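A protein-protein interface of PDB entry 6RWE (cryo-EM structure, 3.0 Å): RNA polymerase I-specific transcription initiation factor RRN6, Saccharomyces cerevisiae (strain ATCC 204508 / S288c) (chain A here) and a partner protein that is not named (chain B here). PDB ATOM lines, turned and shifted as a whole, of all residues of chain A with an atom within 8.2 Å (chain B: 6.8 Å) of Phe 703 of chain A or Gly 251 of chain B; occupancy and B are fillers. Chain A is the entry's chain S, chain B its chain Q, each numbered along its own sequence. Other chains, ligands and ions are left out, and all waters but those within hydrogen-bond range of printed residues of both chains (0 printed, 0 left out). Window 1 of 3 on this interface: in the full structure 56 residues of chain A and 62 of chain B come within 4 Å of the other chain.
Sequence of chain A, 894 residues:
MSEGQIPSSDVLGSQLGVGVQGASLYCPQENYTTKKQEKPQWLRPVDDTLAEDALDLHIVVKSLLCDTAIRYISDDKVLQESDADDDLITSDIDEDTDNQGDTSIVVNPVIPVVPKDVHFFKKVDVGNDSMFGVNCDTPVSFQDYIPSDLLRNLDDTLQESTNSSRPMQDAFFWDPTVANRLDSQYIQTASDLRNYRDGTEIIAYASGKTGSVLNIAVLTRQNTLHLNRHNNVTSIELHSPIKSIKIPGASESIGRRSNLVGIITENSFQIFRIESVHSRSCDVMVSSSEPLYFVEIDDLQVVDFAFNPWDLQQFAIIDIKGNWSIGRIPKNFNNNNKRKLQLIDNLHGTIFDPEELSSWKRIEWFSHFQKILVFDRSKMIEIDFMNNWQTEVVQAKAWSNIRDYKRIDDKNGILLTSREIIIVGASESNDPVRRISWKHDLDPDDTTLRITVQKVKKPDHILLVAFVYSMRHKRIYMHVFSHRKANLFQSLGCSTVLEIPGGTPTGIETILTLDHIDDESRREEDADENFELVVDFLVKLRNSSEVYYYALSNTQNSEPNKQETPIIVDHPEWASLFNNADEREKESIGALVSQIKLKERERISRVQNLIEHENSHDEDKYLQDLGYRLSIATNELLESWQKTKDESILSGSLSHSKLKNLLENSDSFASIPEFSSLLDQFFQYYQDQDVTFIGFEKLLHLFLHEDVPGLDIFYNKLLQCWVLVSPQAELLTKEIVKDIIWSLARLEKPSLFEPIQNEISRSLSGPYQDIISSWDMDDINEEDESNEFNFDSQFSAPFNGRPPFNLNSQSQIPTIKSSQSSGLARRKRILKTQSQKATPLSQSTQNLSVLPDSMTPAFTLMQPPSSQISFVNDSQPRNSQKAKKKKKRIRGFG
The side-chain amide oxygen of Gln 250 of chain B lies within hydrogen-bond range of the side-chain hydroxyl of Ser 743 of chain A, at 3.0 Å. The side-chain carboxylate (OD2) of Asp 739 of chain A is in hydrogen-bond range of the side-chain hydroxyl (OH) of Tyr 267 of chain B (2.6 Å).
The backbone carbonyl oxygen of Asp 739 of chain A lies within hydrogen-bond range of the side-chain hydroxyl of Ser 743 of chain A, 2.8 Å away. The side-chain hydroxyl (OG) of Ser 248 of chain B sits at hydrogen-bond distance from the backbone carbonyl oxygen (O) of Leu 174 of chain B, 3.0 Å away.
Among the printed residues, merely in contact across the chains: Leu 699 of chain A with Leu 174 of chain B (3.7 Å), Leu 702 of chain A with Val 176 of chain B (3.9 Å), Phe 703 of chain A with Pro 175 of chain B (3.6 Å), Phe 703 of chain A with Gly 251 of chain B (3.2 Å), Phe 703 of chain A with Leu 254 of chain B (3.6 Å), Phe 703 of chain A with Phe 438 of chain B (3.8 Å), Leu 704 of chain A with Met 258 of chain B (3.7 Å), Leu 704 of chain A with Ile 439 of chain B (3.8 Å), His 705 of chain A with Phe 438 of chain B (3.8 Å), Glu 706 of chain A with Ile 439 of chain B (3.3 Å), Ile 736 of chain A with Leu 254 of chain B (3.8 Å), Ile 736 of chain A with Tyr 267 of chain B (3.7 Å), Asp 739 of chain A with Gln 250 of chain B (3.6 Å), Ile 740 of chain A with Gln 250 of chain B (3.96 Å) and Ile 740 of chain A with Leu 254 of chain B (3.8 Å).
Printed residues of chain B within 4 Å of Leu 702 of chain A: Val 176. Printed residues of chain B within 4 Å of Phe 703 of chain A: Pro 175 (3.6 Å), Gly 251 (3.2 Å), Leu 254 (3.6 Å) and Phe 438 (3.8 Å). Printed residues of chain B within 4 Å of Asp 739 of chain A: Gln 250 and Tyr 267. Leu 744 of chain A touches none of the printed residues of chain B. Gly 251 of chain B touches one residue of chain A. The nearest residue of chain B that does not touch Phe 703 of chain A is Lys 255 of chain B (4.2 Å).
Printed residues of chain A that touch a printed residue of chain B: Leu 699, Leu 702, Phe 703, Leu 704, His 705, Glu 706, Ile 736, Asp 739, Ile 740 and Ser 743. Hydrophobic or aromatic side chains of chain B within 4 Å of the printed part of chain A: Leu 174, Pro 175, Val 176, Leu 254, Met 258, Tyr 267, Phe 438 and Ile 439.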
ATOM      1  N   LEU A 699     -24.821  -6.286  27.289  1.00  0.00           N
ATOM      2  CA  LEU A 699     -25.090  -7.404  28.184  1.00  0.00           C
ATOM      3  C   LEU A 699     -24.098  -8.548  28.043  1.00  0.00           C
ATOM      4  O   LEU A 699     -23.966  -9.343  28.981  1.00  0.00           O
ATOM      5  CB  LEU A 699     -26.522  -7.923  27.954  1.00  0.00           C
ATOM      6  CG  LEU A 699     -27.218  -8.920  28.887  1.00  0.00           C
ATOM      7  CD1 LEU A 699     -28.686  -8.585  28.949  1.00  0.00           C
ATOM      8  CD2 LEU A 699     -27.059 -10.351  28.408  1.00  0.00           C
ATOM      9  N   LEU A 700     -23.362  -8.629  26.939  1.00  0.00           N
ATOM     10  CA  LEU A 700     -22.422  -9.707  26.653  1.00  0.00           C
ATOM     11  C   LEU A 700     -21.106  -9.566  27.427  1.00  0.00           C
ATOM     12  O   LEU A 700     -20.211 -10.405  27.286  1.00  0.00           O
ATOM     13  CB  LEU A 700     -22.187  -9.748  25.136  1.00  0.00           C
ATOM     14  CG  LEU A 700     -21.462 -10.844  24.352  1.00  0.00           C
ATOM     15  CD1 LEU A 700     -22.123 -12.179  24.588  1.00  0.00           C
ATOM     16  CD2 LEU A 700     -21.504 -10.501  22.882  1.00  0.00           C
ATOM     17  N   HIS A 701     -20.990  -8.549  28.282  1.00  0.00           N
ATOM     18  CA  HIS A 701     -19.791  -8.291  29.070  1.00  0.00           C
ATOM     19  C   HIS A 701     -19.565  -9.294  30.192  1.00  0.00           C
ATOM     20  O   HIS A 701     -18.503  -9.255  30.820  1.00  0.00           O
ATOM     21  CB  HIS A 701     -19.871  -6.888  29.664  1.00  0.00           C
ATOM     22  CG  HIS A 701     -21.037  -6.696  30.578  1.00  0.00           C
ATOM     23  ND1 HIS A 701     -20.983  -6.985  31.924  1.00  0.00           N
ATOM     24  CD2 HIS A 701     -22.297  -6.267  30.335  1.00  0.00           C
ATOM     25  CE1 HIS A 701     -22.156  -6.729  32.474  1.00  0.00           C
ATOM     26  NE2 HIS A 701     -22.971  -6.294  31.531  1.00  0.00           N
ATOM     27  N   LEU A 702     -20.518 -10.189  30.461  1.00  0.00           N
ATOM     28  CA  LEU A 702     -20.342 -11.184  31.511  1.00  0.00           C
ATOM     29  C   LEU A 702     -19.329 -12.260  31.147  1.00  0.00           C
ATOM     30  O   LEU A 702     -18.918 -13.017  32.031  1.00  0.00           O
ATOM     31  CB  LEU A 702     -21.679 -11.842  31.846  1.00  0.00           C
ATOM     32  CG  LEU A 702     -22.753 -10.897  32.382  1.00  0.00           C
ATOM     33  CD1 LEU A 702     -24.028 -11.656  32.693  1.00  0.00           C
ATOM     34  CD2 LEU A 702     -22.261 -10.137  33.592  1.00  0.00           C
ATOM     35  N   PHE A 703     -18.927 -12.355  29.884  1.00  0.00           N
ATOM     36  CA  PHE A 703     -17.883 -13.287  29.485  1.00  0.00           C
ATOM     37  C   PHE A 703     -16.497 -12.662  29.520  1.00  0.00           C
ATOM     38  O   PHE A 703     -15.506 -13.385  29.675  1.00  0.00           O
ATOM     39  CB  PHE A 703     -18.151 -13.808  28.073  1.00  0.00           C
ATOM     40  CG  PHE A 703     -19.399 -14.623  27.952  1.00  0.00           C
ATOM     41  CD1 PHE A 703     -19.403 -15.964  28.292  1.00  0.00           C
ATOM     42  CD2 PHE A 703     -20.569 -14.045  27.492  1.00  0.00           C
ATOM     43  CE1 PHE A 703     -20.551 -16.714  28.171  1.00  0.00           C
ATOM     44  CE2 PHE A 703     -21.720 -14.789  27.374  1.00  0.00           C
ATOM     45  CZ  PHE A 703     -21.710 -16.126  27.712  1.00  0.00           C
ATOM     46  N   LEU A 704     -16.401 -11.339  29.372  1.00  0.00           N
ATOM     47  CA  LEU A 704     -15.113 -10.668  29.299  1.00  0.00           C
ATOM     48  C   LEU A 704     -14.841  -9.718  30.454  1.00  0.00           C
ATOM     49  O   LEU A 704     -13.712  -9.221  30.560  1.00  0.00           O
ATOM     50  CB  LEU A 704     -14.992  -9.897  27.979  1.00  0.00           C
ATOM     51  CG  LEU A 704     -14.964 -10.789  26.741  1.00  0.00           C
ATOM     52  CD1 LEU A 704     -14.887  -9.945  25.485  1.00  0.00           C
ATOM     53  CD2 LEU A 704     -13.803 -11.765  26.810  1.00  0.00           C
ATOM     54  N   HIS A 705     -15.846  -9.441  31.295  1.00  0.00           N
ATOM     55  CA  HIS A 705     -15.713  -8.678  32.542  1.00  0.00           C
ATOM     56  C   HIS A 705     -15.201  -7.257  32.309  1.00  0.00           C
ATOM     57  O   HIS A 705     -14.518  -6.691  33.163  1.00  0.00           O
ATOM     58  CB  HIS A 705     -14.814  -9.401  33.554  1.00  0.00           C
ATOM     59  CG  HIS A 705     -15.309 -10.757  33.951  1.00  0.00           C
ATOM     60  ND1 HIS A 705     -16.380 -10.943  34.797  1.00  0.00           N
ATOM     61  CD2 HIS A 705     -14.865 -11.995  33.630  1.00  0.00           C
ATOM     62  CE1 HIS A 705     -16.581 -12.237  34.971  1.00  0.00           C
ATOM     63  NE2 HIS A 705     -15.675 -12.897  34.273  1.00  0.00           N
ATOM     64  N   GLU A 706     -15.515  -6.664  31.161  1.00  0.00           N
ATOM     65  CA  GLU A 706     -15.013  -5.334  30.844  1.00  0.00           C
ATOM     66  C   GLU A 706     -16.016  -4.614  29.948  1.00  0.00           C
ATOM     67  O   GLU A 706     -17.142  -5.079  29.743  1.00  0.00           O
ATOM     68  CB  GLU A 706     -13.637  -5.411  30.175  1.00  0.00           C
ATOM     69  CG  GLU A 706     -13.665  -6.059  28.806  1.00  0.00           C
ATOM     70  CD  GLU A 706     -12.340  -5.967  28.104  1.00  0.00           C
ATOM     71  OE1 GLU A 706     -11.380  -5.456  28.719  1.00  0.00           O
ATOM     72  OE2 GLU A 706     -12.274  -6.377  26.927  1.00  0.00           O
ATOM     73  N   VAL A 708     -17.740  -3.675  26.690  1.00  0.00           N
ATOM     74  CA  VAL A 708     -18.031  -4.245  25.382  1.00  0.00           C
ATOM     75  C   VAL A 708     -18.769  -3.191  24.564  1.00  0.00           C
ATOM     76  O   VAL A 708     -19.973  -2.985  24.735  1.00  0.00           O
ATOM     77  CB  VAL A 708     -18.850  -5.545  25.497  1.00  0.00           C
ATOM     78  CG1 VAL A 708     -19.199  -6.091  24.116  1.00  0.00           C
ATOM     79  CG2 VAL A 708     -18.071  -6.584  26.268  1.00  0.00           C
ATOM     80  N   PHE A 714     -16.536  -8.028  20.068  1.00  0.00           N
ATOM     81  CA  PHE A 714     -16.530  -9.171  20.970  1.00  0.00           C
ATOM     82  C   PHE A 714     -15.763 -10.327  20.350  1.00  0.00           C
ATOM     83  O   PHE A 714     -15.028 -11.039  21.041  1.00  0.00           O
ATOM     84  CB  PHE A 714     -17.963  -9.588  21.287  1.00  0.00           C
ATOM     85  CG  PHE A 714     -18.065 -10.778  22.192  1.00  0.00           C
ATOM     86  CD1 PHE A 714     -17.840 -10.647  23.551  1.00  0.00           C
ATOM     87  CD2 PHE A 714     -18.398 -12.025  21.687  1.00  0.00           C
ATOM     88  CE1 PHE A 714     -17.935 -11.739  24.395  1.00  0.00           C
ATOM     89  CE2 PHE A 714     -18.495 -13.121  22.523  1.00  0.00           C
ATOM     90  CZ  PHE A 714     -18.264 -12.976  23.880  1.00  0.00           C
ATOM     91  N   LEU A 718     -12.000 -12.463  21.149  1.00  0.00           N
ATOM     92  CA  LEU A 718     -12.023 -13.918  21.103  1.00  0.00           C
ATOM     93  C   LEU A 718     -11.281 -14.490  19.903  1.00  0.00           C
ATOM     94  O   LEU A 718     -10.832 -15.639  19.971  1.00  0.00           O
ATOM     95  CB  LEU A 718     -13.461 -14.449  21.103  1.00  0.00           C
ATOM     96  CG  LEU A 718     -14.120 -14.723  22.457  1.00  0.00           C
ATOM     97  CD1 LEU A 718     -14.486 -13.447  23.192  1.00  0.00           C
ATOM     98  CD2 LEU A 718     -15.342 -15.614  22.276  1.00  0.00           C
ATOM     99  N   ILE A 736     -18.717 -20.396  17.909  1.00  0.00           N
ATOM    100  CA  ILE A 736     -19.054 -20.170  19.310  1.00  0.00           C
ATOM    101  C   ILE A 736     -19.803 -18.851  19.460  1.00  0.00           C
ATOM    102  O   ILE A 736     -20.761 -18.749  20.238  1.00  0.00           O
ATOM    103  CB  ILE A 736     -17.783 -20.211  20.178  1.00  0.00           C
ATOM    104  CG1 ILE A 736     -17.121 -21.578  20.083  1.00  0.00           C
ATOM    105  CG2 ILE A 736     -18.106 -19.941  21.635  1.00  0.00           C
ATOM    106  CD1 ILE A 736     -15.733 -21.628  20.668  1.00  0.00           C
ATOM    107  N   ASP A 739     -23.119 -19.561  18.460  1.00  0.00           N
ATOM    108  CA  ASP A 739     -23.813 -20.373  19.451  1.00  0.00           C
ATOM    109  C   ASP A 739     -24.252 -19.532  20.642  1.00  0.00           C
ATOM    110  O   ASP A 739     -25.204 -19.895  21.337  1.00  0.00           O
ATOM    111  CB  ASP A 739     -22.916 -21.521  19.903  1.00  0.00           C
ATOM    112  CG  ASP A 739     -23.695 -22.658  20.538  1.00  0.00           C
ATOM    113  OD1 ASP A 739     -24.941 -22.608  20.579  1.00  0.00           O
ATOM    114  OD2 ASP A 739     -23.049 -23.617  21.002  1.00  0.00           O
ATOM    115  N   ILE A 740     -23.587 -18.402  20.882  1.00  0.00           N
ATOM    116  CA  ILE A 740     -24.046 -17.476  21.912  1.00  0.00           C
ATOM    117  C   ILE A 740     -25.299 -16.742  21.452  1.00  0.00           C
ATOM    118  O   ILE A 740     -26.311 -16.713  22.161  1.00  0.00           O
ATOM    119  CB  ILE A 740     -22.925 -16.498  22.296  1.00  0.00           C
ATOM    120  CG1 ILE A 740     -21.807 -17.250  23.013  1.00  0.00           C
ATOM    121  CG2 ILE A 740     -23.460 -15.371  23.158  1.00  0.00           C
ATOM    122  CD1 ILE A 740     -22.279 -17.948  24.286  1.00  0.00           C
ATOM    123  N   ILE A 741     -25.252 -16.152  20.254  1.00  0.00           N
ATOM    124  CA  ILE A 741     -26.358 -15.325  19.777  1.00  0.00           C
ATOM    125  C   ILE A 741     -27.574 -16.191  19.459  1.00  0.00           C
ATOM    126  O   ILE A 741     -28.720 -15.742  19.593  1.00  0.00           O
ATOM    127  CB  ILE A 741     -25.892 -14.485  18.570  1.00  0.00           C
ATOM    128  CG1 ILE A 741     -24.633 -13.701  18.936  1.00  0.00           C
ATOM    129  CG2 ILE A 741     -26.948 -13.476  18.141  1.00  0.00           C
ATOM    130  CD1 ILE A 741     -24.820 -12.756  20.100  1.00  0.00           C
ATOM    131  N   SER A 743     -28.218 -18.611  21.432  1.00  0.00           N
ATOM    132  CA  SER A 743     -28.674 -18.976  22.765  1.00  0.00           C
ATOM    133  C   SER A 743     -29.096 -17.780  23.596  1.00  0.00           C
ATOM    134  O   SER A 743     -29.941 -17.927  24.482  1.00  0.00           O
ATOM    135  CB  SER A 743     -27.582 -19.742  23.529  1.00  0.00           C
ATOM    136  OG  SER A 743     -27.282 -20.967  22.883  1.00  0.00           O
ATOM    137  N   LEU A 744     -28.550 -16.596  23.323  1.00  0.00           N
ATOM    138  CA  LEU A 744     -28.896 -15.381  24.043  1.00  0.00           C
ATOM    139  C   LEU A 744     -30.096 -14.685  23.405  1.00  0.00           C
ATOM    140  O   LEU A 744     -30.408 -13.543  23.752  1.00  0.00           O
ATOM    141  CB  LEU A 744     -27.664 -14.461  24.101  1.00  0.00           C
ATOM    142  CG  LEU A 744     -27.340 -13.476  25.240  1.00  0.00           C
ATOM    143  CD1 LEU A 744     -25.830 -13.386  25.354  1.00  0.00           C
ATOM    144  CD2 LEU A 744     -27.894 -12.073  25.119  1.00  0.00           C
ATOM    145  N   LEU B 174     -30.149 -15.505  31.051  1.00  0.00           N
ATOM    146  CA  LEU B 174     -28.881 -14.810  31.125  1.00  0.00           C
ATOM    147  C   LEU B 174     -27.733 -15.791  31.347  1.00  0.00           C
ATOM    148  O   LEU B 174     -27.939 -16.881  31.889  1.00  0.00           O
ATOM    149  CB  LEU B 174     -28.905 -13.791  32.269  1.00  0.00           C
ATOM    150  CG  LEU B 174     -29.873 -12.631  32.084  1.00  0.00           C
ATOM    151  CD1 LEU B 174     -29.998 -11.870  33.375  1.00  0.00           C
ATOM    152  CD2 LEU B 174     -29.385 -11.715  30.983  1.00  0.00           C
ATOM    153  N   PRO B 175     -26.503 -15.432  30.942  1.00  0.00           N
ATOM    154  CA  PRO B 175     -25.347 -16.290  31.243  1.00  0.00           C
ATOM    155  C   PRO B 175     -24.774 -16.101  32.643  1.00  0.00           C
ATOM    156  O   PRO B 175     -23.619 -16.457  32.894  1.00  0.00           O
ATOM    157  CB  PRO B 175     -24.327 -15.880  30.174  1.00  0.00           C
ATOM    158  CG  PRO B 175     -24.675 -14.478  29.850  1.00  0.00           C
ATOM    159  CD  PRO B 175     -26.169 -14.392  29.952  1.00  0.00           C
ATOM    160  N   VAL B 176     -25.545 -15.510  33.549  1.00  0.00           N
ATOM    161  CA  VAL B 176     -25.127 -15.300  34.929  1.00  0.00           C
ATOM    162  C   VAL B 176     -25.632 -16.474  35.764  1.00  0.00           C
ATOM    163  O   VAL B 176     -26.689 -17.051  35.476  1.00  0.00           O
ATOM    164  CB  VAL B 176     -25.628 -13.930  35.442  1.00  0.00           C
ATOM    165  CG1 VAL B 176     -27.144 -13.870  35.551  1.00  0.00           C
ATOM    166  CG2 VAL B 176     -24.962 -13.539  36.752  1.00  0.00           C
ATOM    167  N   TYR B 177     -24.838 -16.881  36.755  1.00  0.00           N
ATOM    168  CA  TYR B 177     -25.126 -18.095  37.512  1.00  0.00           C
ATOM    169  C   TYR B 177     -24.840 -17.932  38.996  1.00  0.00           C
ATOM    170  O   TYR B 177     -24.579 -16.822  39.468  1.00  0.00           O
ATOM    171  CB  TYR B 177     -24.294 -19.259  36.985  1.00  0.00           C
ATOM    172  CG  TYR B 177     -24.646 -19.661  35.590  1.00  0.00           C
ATOM    173  CD1 TYR B 177     -25.746 -20.466  35.338  1.00  0.00           C
ATOM    174  CD2 TYR B 177     -23.885 -19.225  34.519  1.00  0.00           C
ATOM    175  CE1 TYR B 177     -26.073 -20.826  34.054  1.00  0.00           C
ATOM    176  CE2 TYR B 177     -24.205 -19.577  33.239  1.00  0.00           C
ATOM    177  CZ  TYR B 177     -25.295 -20.379  33.010  1.00  0.00           C
ATOM    178  OH  TYR B 177     -25.606 -20.728  31.723  1.00  0.00           O
ATOM    179  N   ASP B 180     -21.471 -16.718  39.282  1.00  0.00           N
ATOM    180  CA  ASP B 180     -21.425 -15.263  39.288  1.00  0.00           C
ATOM    181  C   ASP B 180     -22.443 -14.658  40.243  1.00  0.00           C
ATOM    182  O   ASP B 180     -22.880 -13.523  40.051  1.00  0.00           O
ATOM    183  CB  ASP B 180     -21.628 -14.712  37.879  1.00  0.00           C
ATOM    184  CG  ASP B 180     -20.424 -14.921  36.995  1.00  0.00           C
ATOM    185  OD1 ASP B 180     -19.297 -14.973  37.533  1.00  0.00           O
ATOM    186  OD2 ASP B 180     -20.599 -15.027  35.763  1.00  0.00           O
ATOM    187  N   SER B 248     -29.365 -21.602  30.308  1.00  0.00           N
ATOM    188  CA  SER B 248     -28.583 -21.276  29.126  1.00  0.00           C
ATOM    189  C   SER B 248     -27.205 -21.907  29.256  1.00  0.00           C
ATOM    190  O   SER B 248     -26.231 -21.231  29.596  1.00  0.00           O
ATOM    191  CB  SER B 248     -28.481 -19.761  28.941  1.00  0.00           C
ATOM    192  OG  SER B 248     -27.735 -19.165  29.986  1.00  0.00           O
ATOM    193  N   CYS B 249     -27.116 -23.202  28.962  1.00  0.00           N
ATOM    194  CA  CYS B 249     -25.905 -23.970  29.201  1.00  0.00           C
ATOM    195  C   CYS B 249     -24.811 -23.669  28.195  1.00  0.00           C
ATOM    196  O   CYS B 249     -23.671 -24.094  28.396  1.00  0.00           O
ATOM    197  CB  CYS B 249     -26.234 -25.460  29.186  1.00  0.00           C
ATOM    198  SG  CYS B 249     -27.448 -25.896  30.439  1.00  0.00           S
ATOM    199  N   GLN B 250     -25.127 -22.944  27.130  1.00  0.00           N
ATOM    200  CA  GLN B 250     -24.112 -22.485  26.198  1.00  0.00           C
ATOM    201  C   GLN B 250     -23.327 -21.302  26.747  1.00  0.00           C
ATOM    202  O   GLN B 250     -22.114 -21.214  26.522  1.00  0.00           O
ATOM    203  CB  GLN B 250     -24.764 -22.125  24.859  1.00  0.00           C
ATOM    204  CG  GLN B 250     -25.332 -23.332  24.102  1.00  0.00           C
ATOM    205  CD  GLN B 250     -26.746 -23.710  24.532  1.00  0.00           C
ATOM    206  OE1 GLN B 250     -27.461 -22.903  25.124  1.00  0.00           O
ATOM    207  NE2 GLN B 250     -27.144 -24.945  24.249  1.00  0.00           N
ATOM    208  N   GLY B 251     -23.985 -20.403  27.477  1.00  0.00           N
ATOM    209  CA  GLY B 251     -23.287 -19.338  28.178  1.00  0.00           C
ATOM    210  C   GLY B 251     -22.601 -19.769  29.453  1.00  0.00           C
ATOM    211  O   GLY B 251     -21.852 -18.983  30.042  1.00  0.00           O
ATOM    212  N   LEU B 252     -22.845 -21.001  29.894  1.00  0.00           N
ATOM    213  CA  LEU B 252     -22.151 -21.530  31.059  1.00  0.00           C
ATOM    214  C   LEU B 252     -20.751 -21.987  30.687  1.00  0.00           C
ATOM    215  O   LEU B 252     -19.770 -21.586  31.322  1.00  0.00           O
ATOM    216  CB  LEU B 252     -22.956 -22.687  31.660  1.00  0.00           C
ATOM    217  CG  LEU B 252     -22.647 -23.253  33.050  1.00  0.00           C
ATOM    218  CD1 LEU B 252     -23.938 -23.743  33.681  1.00  0.00           C
ATOM    219  CD2 LEU B 252     -21.646 -24.392  33.015  1.00  0.00           C
ATOM    220  N   LEU B 253     -20.646 -22.823  29.655  1.00  0.00           N
ATOM    221  CA  LEU B 253     -19.382 -23.474  29.346  1.00  0.00           C
ATOM    222  C   LEU B 253     -18.391 -22.535  28.680  1.00  0.00           C
ATOM    223  O   LEU B 253     -17.186 -22.797  28.729  1.00  0.00           O
ATOM    224  CB  LEU B 253     -19.630 -24.691  28.460  1.00  0.00           C
ATOM    225  CG  LEU B 253     -20.439 -25.780  29.154  1.00  0.00           C
ATOM    226  CD1 LEU B 253     -20.763 -26.893  28.179  1.00  0.00           C
ATOM    227  CD2 LEU B 253     -19.674 -26.306  30.356  1.00  0.00           C
ATOM    228  N   LEU B 254     -18.867 -21.449  28.060  1.00  0.00           N
ATOM    229  CA  LEU B 254     -17.946 -20.468  27.497  1.00  0.00           C
ATOM    230  C   LEU B 254     -17.143 -19.772  28.588  1.00  0.00           C
ATOM    231  O   LEU B 254     -15.964 -19.453  28.388  1.00  0.00           O
ATOM    232  CB  LEU B 254     -18.704 -19.447  26.647  1.00  0.00           C
ATOM    233  CG  LEU B 254     -17.814 -18.421  25.943  1.00  0.00           C
ATOM    234  CD1 LEU B 254     -16.782 -19.138  25.082  1.00  0.00           C
ATOM    235  CD2 LEU B 254     -18.631 -17.452  25.105  1.00  0.00           C
ATOM    236  N   LYS B 255     -17.746 -19.563  29.758  1.00  0.00           N
ATOM    237  CA  LYS B 255     -16.961 -19.168  30.918  1.00  0.00           C
ATOM    238  C   LYS B 255     -16.031 -20.298  31.341  1.00  0.00           C
ATOM    239  O   LYS B 255     -14.852 -20.072  31.625  1.00  0.00           O
ATOM    240  CB  LYS B 255     -17.874 -18.754  32.072  1.00  0.00           C
ATOM    241  CG  LYS B 255     -17.101 -18.193  33.250  1.00  0.00           C
ATOM    242  CD  LYS B 255     -17.998 -17.784  34.406  1.00  0.00           C
ATOM    243  CE  LYS B 255     -17.150 -17.286  35.570  1.00  0.00           C
ATOM    244  NZ  LYS B 255     -17.943 -16.947  36.783  1.00  0.00           N
ATOM    245  N   LEU B 256     -16.540 -21.535  31.350  1.00  0.00           N
ATOM    246  CA  LEU B 256     -15.726 -22.688  31.731  1.00  0.00           C
ATOM    247  C   LEU B 256     -14.672 -23.045  30.690  1.00  0.00           C
ATOM    248  O   LEU B 256     -13.727 -23.772  31.012  1.00  0.00           O
ATOM    249  CB  LEU B 256     -16.613 -23.905  31.998  1.00  0.00           C
ATOM    250  CG  LEU B 256     -17.160 -24.127  33.413  1.00  0.00           C
ATOM    251  CD1 LEU B 256     -18.227 -23.121  33.809  1.00  0.00           C
ATOM    252  CD2 LEU B 256     -17.687 -25.550  33.550  1.00  0.00           C
ATOM    253  N   MET B 258     -13.010 -20.419  29.019  1.00  0.00           N
ATOM    254  CA  MET B 258     -12.060 -19.347  29.273  1.00  0.00           C
ATOM    255  C   MET B 258     -11.584 -19.307  30.719  1.00  0.00           C
ATOM    256  O   MET B 258     -10.755 -18.457  31.056  1.00  0.00           O
ATOM    257  CB  MET B 258     -12.692 -18.007  28.897  1.00  0.00           C
ATOM    258  CG  MET B 258     -13.102 -17.925  27.437  1.00  0.00           C
ATOM    259  SD  MET B 258     -13.911 -16.377  26.995  1.00  0.00           S
ATOM    260  CE  MET B 258     -12.507 -15.270  27.003  1.00  0.00           C
ATOM    261  N   TYR B 267     -15.263 -27.015  23.707  1.00  0.00           N
ATOM    262  CA  TYR B 267     -16.621 -26.502  23.808  1.00  0.00           C
ATOM    263  C   TYR B 267     -17.592 -27.364  23.012  1.00  0.00           C
ATOM    264  O   TYR B 267     -18.730 -27.588  23.440  1.00  0.00           O
ATOM    265  CB  TYR B 267     -16.678 -25.048  23.341  1.00  0.00           C
ATOM    266  CG  TYR B 267     -18.084 -24.509  23.345  1.00  0.00           C
ATOM    267  CD1 TYR B 267     -18.761 -24.298  24.537  1.00  0.00           C
ATOM    268  CD2 TYR B 267     -18.737 -24.216  22.159  1.00  0.00           C
ATOM    269  CE1 TYR B 267     -20.057 -23.815  24.546  1.00  0.00           C
ATOM    270  CE2 TYR B 267     -20.026 -23.730  22.155  1.00  0.00           C
ATOM    271  CZ  TYR B 267     -20.682 -23.531  23.351  1.00  0.00           C
ATOM    272  OH  TYR B 267     -21.967 -23.048  23.351  1.00  0.00           O
ATOM    273  N   PHE B 438      -9.066  -9.749  32.528  1.00  0.00           N
ATOM    274  CA  PHE B 438      -9.349 -11.145  32.215  1.00  0.00           C
ATOM    275  C   PHE B 438      -9.194 -11.458  30.734  1.00  0.00           C
ATOM    276  O   PHE B 438      -8.989 -12.621  30.371  1.00  0.00           O
ATOM    277  CB  PHE B 438     -10.766 -11.495  32.688  1.00  0.00           C
ATOM    278  CG  PHE B 438     -11.130 -12.938  32.511  1.00  0.00           C
ATOM    279  CD1 PHE B 438     -10.621 -13.905  33.362  1.00  0.00           C
ATOM    280  CD2 PHE B 438     -11.975 -13.328  31.488  1.00  0.00           C
ATOM    281  CE1 PHE B 438     -10.952 -15.238  33.196  1.00  0.00           C
ATOM    282  CE2 PHE B 438     -12.307 -14.657  31.317  1.00  0.00           C
ATOM    283  CZ  PHE B 438     -11.796 -15.612  32.173  1.00  0.00           C
ATOM    284  N   ILE B 439      -9.277 -10.449  29.867  1.00  0.00           N
ATOM    285  CA  ILE B 439      -9.028 -10.673  28.445  1.00  0.00           C
ATOM    286  C   ILE B 439      -7.552 -10.823  28.129  1.00  0.00           C
ATOM    287  O   ILE B 439      -7.210 -11.304  27.042  1.00  0.00           O
ATOM    288  CB  ILE B 439      -9.587  -9.519  27.595  1.00  0.00           C
ATOM    289  CG1 ILE B 439      -8.878  -8.214  27.959  1.00  0.00           C
ATOM    290  CG2 ILE B 439     -11.077  -9.381  27.815  1.00  0.00           C
ATOM    291  CD1 ILE B 439      -9.067  -7.096  26.979  1.00  0.00           C
